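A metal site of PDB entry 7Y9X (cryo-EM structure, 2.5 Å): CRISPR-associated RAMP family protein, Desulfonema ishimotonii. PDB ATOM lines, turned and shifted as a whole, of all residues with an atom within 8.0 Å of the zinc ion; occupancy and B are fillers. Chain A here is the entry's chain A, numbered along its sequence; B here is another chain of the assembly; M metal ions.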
ATOM      1  N   ARG A 452      -4.728   0.611 -25.178  1.00  0.00           N
ATOM      2  CA  ARG A 452      -5.054   2.038 -25.209  1.00  0.00           C
ATOM      3  C   ARG A 452      -6.078   2.387 -24.146  1.00  0.00           C
ATOM      4  O   ARG A 452      -5.956   3.420 -23.471  1.00  0.00           O
ATOM      5  CB  ARG A 452      -5.570   2.427 -26.604  1.00  0.00           C
ATOM      6  CG  ARG A 452      -5.920   3.886 -26.738  1.00  0.00           C
ATOM      7  CD  ARG A 452      -6.400   4.226 -28.131  1.00  0.00           C
ATOM      8  NE  ARG A 452      -5.387   3.981 -29.153  1.00  0.00           N
ATOM      9  CZ  ARG A 452      -4.459   4.857 -29.502  1.00  0.00           C
ATOM     10  NH1 ARG A 452      -4.360   6.039 -28.910  1.00  0.00           N
ATOM     11  NH2 ARG A 452      -3.613   4.556 -30.483  1.00  0.00           N
ATOM     12  N   GLN A 456      -5.169   4.783 -20.759  1.00  0.00           N
ATOM     13  CA  GLN A 456      -6.001   5.910 -20.354  1.00  0.00           C
ATOM     14  C   GLN A 456      -6.573   5.709 -18.963  1.00  0.00           C
ATOM     15  O   GLN A 456      -6.824   6.689 -18.261  1.00  0.00           O
ATOM     16  CB  GLN A 456      -7.127   6.121 -21.356  1.00  0.00           C
ATOM     17  CG  GLN A 456      -6.656   6.434 -22.759  1.00  0.00           C
ATOM     18  CD  GLN A 456      -7.806   6.621 -23.716  1.00  0.00           C
ATOM     19  OE1 GLN A 456      -8.706   7.405 -23.463  1.00  0.00           O
ATOM     20  NE2 GLN A 456      -7.775   5.883 -24.806  1.00  0.00           N
ATOM     21  N   SER A 461      -6.979   9.815 -17.798  1.00  0.00           N
ATOM     22  CA  SER A 461      -7.092  10.922 -18.745  1.00  0.00           C
ATOM     23  C   SER A 461      -7.664  10.409 -20.056  1.00  0.00           C
ATOM     24  O   SER A 461      -6.954   9.769 -20.842  1.00  0.00           O
ATOM     25  CB  SER A 461      -5.741  11.590 -18.978  1.00  0.00           C
ATOM     26  OG  SER A 461      -5.199  12.099 -17.774  1.00  0.00           O
ATOM     27  N   PRO A 462      -8.946  10.668 -20.323  1.00  0.00           N
ATOM     28  CA  PRO A 462      -9.499  10.347 -21.636  1.00  0.00           C
ATOM     29  C   PRO A 462      -8.792  11.133 -22.732  1.00  0.00           C
ATOM     30  O   PRO A 462      -8.379  12.274 -22.538  1.00  0.00           O
ATOM     31  CB  PRO A 462     -10.961  10.767 -21.520  1.00  0.00           C
ATOM     32  CG  PRO A 462     -11.245  10.633 -20.070  1.00  0.00           C
ATOM     33  CD  PRO A 462      -9.991  11.138 -19.401  1.00  0.00           C
ATOM     34  N   CYS A 463      -8.655  10.504 -23.893  1.00  0.00           N
ATOM     35  CA  CYS A 463      -8.146  11.158 -25.080  1.00  0.00           C
ATOM     36  C   CYS A 463      -9.328  11.542 -25.974  1.00  0.00           C
ATOM     37  O   CYS A 463     -10.152  10.694 -26.303  1.00  0.00           O
ATOM     38  CB  CYS A 463      -7.191  10.254 -25.841  1.00  0.00           C
ATOM     39  SG  CYS A 463      -6.450  11.029 -27.283  1.00  0.00           S
ATOM     40  N   ASN A 464      -9.392  12.820 -26.346  1.00  0.00           N
ATOM     41  CA  ASN A 464     -10.465  13.316 -27.199  1.00  0.00           C
ATOM     42  C   ASN A 464      -9.980  13.599 -28.611  1.00  0.00           C
ATOM     43  O   ASN A 464     -10.611  14.378 -29.338  1.00  0.00           O
ATOM     44  CB  ASN A 464     -11.095  14.580 -26.583  1.00  0.00           C
ATOM     45  CG  ASN A 464     -10.124  15.734 -26.498  1.00  0.00           C
ATOM     46  OD1 ASN A 464      -8.923  15.575 -26.658  1.00  0.00           O
ATOM     47  ND2 ASN A 464     -10.658  16.922 -26.246  1.00  0.00           N
ATOM     48  N   ALA A 465      -8.875  12.981 -29.019  1.00  0.00           N
ATOM     49  CA  ALA A 465      -8.363  13.193 -30.365  1.00  0.00           C
ATOM     50  C   ALA A 465      -9.316  12.636 -31.408  1.00  0.00           C
ATOM     51  O   ALA A 465     -10.013  11.637 -31.188  1.00  0.00           O
ATOM     52  CB  ALA A 465      -6.980  12.548 -30.513  1.00  0.00           C
ATOM     53  N   GLU A 466      -9.351  13.291 -32.558  1.00  0.00           N
ATOM     54  CA  GLU A 466     -10.170  12.885 -33.678  1.00  0.00           C
ATOM     55  C   GLU A 466      -9.299  12.208 -34.726  1.00  0.00           C
ATOM     56  O   GLU A 466      -8.082  12.381 -34.758  1.00  0.00           O
ATOM     57  CB  GLU A 466     -10.887  14.093 -34.289  1.00  0.00           C
ATOM     58  CG  GLU A 466     -11.815  14.811 -33.321  1.00  0.00           C
ATOM     59  CD  GLU A 466     -13.060  14.010 -33.013  1.00  0.00           C
ATOM     60  OE1 GLU A 466     -13.453  13.169 -33.854  1.00  0.00           O
ATOM     61  OE2 GLU A 466     -13.634  14.205 -31.933  1.00  0.00           O
ATOM     62  N   PRO A 471      -0.450  13.787 -35.105  1.00  0.00           N
ATOM     63  CA  PRO A 471      -0.662  12.792 -34.051  1.00  0.00           C
ATOM     64  C   PRO A 471      -0.846  13.447 -32.687  1.00  0.00           C
ATOM     65  O   PRO A 471      -0.192  14.435 -32.347  1.00  0.00           O
ATOM     66  CB  PRO A 471       0.604  11.941 -34.097  1.00  0.00           C
ATOM     67  CG  PRO A 471       1.122  12.116 -35.461  1.00  0.00           C
ATOM     68  CD  PRO A 471       0.785  13.514 -35.861  1.00  0.00           C
ATOM     69  N   CYS A 472      -1.745  12.876 -31.898  1.00  0.00           N
ATOM     70  CA  CYS A 472      -2.016  13.412 -30.575  1.00  0.00           C
ATOM     71  C   CYS A 472      -0.820  13.201 -29.660  1.00  0.00           C
ATOM     72  O   CYS A 472      -0.123  12.196 -29.733  1.00  0.00           O
ATOM     73  CB  CYS A 472      -3.273  12.773 -29.990  1.00  0.00           C
ATOM     74  SG  CYS A 472      -3.515  13.143 -28.260  1.00  0.00           S
ATOM     75  N   MET A 473      -0.601  14.178 -28.776  1.00  0.00           N
ATOM     76  CA  MET A 473       0.594  14.222 -27.937  1.00  0.00           C
ATOM     77  C   MET A 473       0.305  13.911 -26.479  1.00  0.00           C
ATOM     78  O   MET A 473       1.124  14.257 -25.616  1.00  0.00           O
ATOM     79  CB  MET A 473       1.274  15.578 -28.068  1.00  0.00           C
ATOM     80  CG  MET A 473       2.003  15.769 -29.371  1.00  0.00           C
ATOM     81  SD  MET A 473       3.307  14.540 -29.585  1.00  0.00           S
ATOM     82  CE  MET A 473       3.775  14.847 -31.270  1.00  0.00           C
ATOM     83  N   CYS A 474      -0.819  13.276 -26.168  1.00  0.00           N
ATOM     84  CA  CYS A 474      -1.030  12.858 -24.797  1.00  0.00           C
ATOM     85  C   CYS A 474      -0.155  11.653 -24.482  1.00  0.00           C
ATOM     86  O   CYS A 474       0.427  11.009 -25.357  1.00  0.00           O
ATOM     87  CB  CYS A 474      -2.501  12.541 -24.527  1.00  0.00           C
ATOM     88  SG  CYS A 474      -3.163  11.025 -25.248  1.00  0.00           S
ATOM     89  N   LYS A 475      -0.067  11.339 -23.188  1.00  0.00           N
ATOM     90  CA  LYS A 475       0.798  10.268 -22.724  1.00  0.00           C
ATOM     91  C   LYS A 475       0.370   8.921 -23.281  1.00  0.00           C
ATOM     92  O   LYS A 475       1.223   8.075 -23.584  1.00  0.00           O
ATOM     93  CB  LYS A 475       0.811  10.253 -21.201  1.00  0.00           C
ATOM     94  CG  LYS A 475       1.268  11.558 -20.572  1.00  0.00           C
ATOM     95  CD  LYS A 475       1.080  11.537 -19.071  1.00  0.00           C
ATOM     96  CE  LYS A 475       1.478  12.867 -18.460  1.00  0.00           C
ATOM     97  NZ  LYS A 475       1.281  12.893 -16.983  1.00  0.00           N
ATOM     98  N   THR A 476      -0.932   8.688 -23.417  1.00  0.00           N
ATOM     99  CA  THR A 476      -1.417   7.427 -23.957  1.00  0.00           C
ATOM    100  C   THR A 476      -1.040   7.255 -25.425  1.00  0.00           C
ATOM    101  O   THR A 476      -0.550   6.193 -25.837  1.00  0.00           O
ATOM    102  CB  THR A 476      -2.927   7.312 -23.784  1.00  0.00           C
ATOM    103  OG1 THR A 476      -3.260   7.385 -22.391  1.00  0.00           O
ATOM    104  CG2 THR A 476      -3.434   5.999 -24.347  1.00  0.00           C
ATOM    105  N   CYS A 477      -1.261   8.296 -26.235  1.00  0.00           N
ATOM    106  CA  CYS A 477      -1.017   8.175 -27.666  1.00  0.00           C
ATOM    107  C   CYS A 477       0.469   8.049 -27.974  1.00  0.00           C
ATOM    108  O   CYS A 477       0.849   7.427 -28.965  1.00  0.00           O
ATOM    109  CB  CYS A 477      -1.610   9.380 -28.409  1.00  0.00           C
ATOM    110  SG  CYS A 477      -3.392   9.312 -28.661  1.00  0.00           S
ATOM    111  N   ARG A 478       1.323   8.675 -27.162  1.00  0.00           N
ATOM    112  CA  ARG A 478       2.758   8.568 -27.407  1.00  0.00           C
ATOM    113  C   ARG A 478       3.293   7.201 -27.017  1.00  0.00           C
ATOM    114  O   ARG A 478       4.229   6.694 -27.643  1.00  0.00           O
ATOM    115  CB  ARG A 478       3.503   9.683 -26.664  1.00  0.00           C
ATOM    116  CG  ARG A 478       3.281  11.054 -27.284  1.00  0.00           C
ATOM    117  CD  ARG A 478       4.142  12.143 -26.679  1.00  0.00           C
ATOM    118  NE  ARG A 478       3.670  12.588 -25.381  1.00  0.00           N
ATOM    119  CZ  ARG A 478       4.270  12.326 -24.227  1.00  0.00           C
ATOM    120  NH1 ARG A 478       5.395  11.631 -24.176  1.00  0.00           N
ATOM    121  NH2 ARG A 478       3.734  12.789 -23.096  1.00  0.00           N
ATOM    122  N   ARG A 481       2.187   4.695 -29.740  1.00  0.00           N
ATOM    123  CA  ARG A 481       2.996   4.769 -30.948  1.00  0.00           C
ATOM    124  C   ARG A 481       4.335   4.067 -30.793  1.00  0.00           C
ATOM    125  O   ARG A 481       5.051   3.932 -31.790  1.00  0.00           O
ATOM    126  CB  ARG A 481       3.204   6.224 -31.361  1.00  0.00           C
ATOM    127  CG  ARG A 481       1.975   6.878 -31.954  1.00  0.00           C
ATOM    128  CD  ARG A 481       2.309   8.145 -32.723  1.00  0.00           C
ATOM    129  NE  ARG A 481       2.775   9.218 -31.850  1.00  0.00           N
ATOM    130  CZ  ARG A 481       1.990  10.094 -31.253  1.00  0.00           C
ATOM    131  NH1 ARG A 481       0.672  10.045 -31.385  1.00  0.00           N
ATOM    132  NH2 ARG A 481       2.524  11.036 -30.494  1.00  0.00           N
ATOM    133  N   MET B 620      -7.935  16.898 -21.094  1.00  0.00           N
ATOM    134  CA  MET B 620      -8.140  17.506 -22.407  1.00  0.00           C
ATOM    135  C   MET B 620      -9.612  17.770 -22.658  1.00  0.00           C
ATOM    136  O   MET B 620      -9.970  18.802 -23.243  1.00  0.00           O
ATOM    137  CB  MET B 620      -7.583  16.606 -23.507  1.00  0.00           C
ATOM    138  CG  MET B 620      -6.133  16.232 -23.354  1.00  0.00           C
ATOM    139  SD  MET B 620      -5.602  15.132 -24.684  1.00  0.00           S
ATOM    140  CE  MET B 620      -3.914  15.686 -24.895  1.00  0.00           C
HETATM  141 ZN    ZN M   1      -4.129  11.102 -27.361  1.00  0.00          ZN
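The backbone carbonyl oxygen (O) of Cys 472 sits at hydrogen-bond distance from the guanidinium group (NH1) of Arg 481 (2.8 Å).
The side-chain sulfur (SG) of Cys 474 sits close to the backbone NH (N) of Thr 476.
The guanidinium group (NH1) of Arg 452 sits close to the side-chain sulfur (SG) of Cys 477 (3.4 Å).
The side-chain sulfur of Cys 463 sits close to the backbone NH of Ala 465 (3.6 Å).
The backbone NH of Cys 463 sits at hydrogen-bond distance from the side-chain amide oxygen of Gln 456 (3.1 Å).
The zinc ion is bound by SG of Cys 472 (2.3 Å), SG of Cys 463 (2.3 Å), SG of Cys 474 (2.3 Å) and SG of Cys 477 (2.3 Å).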
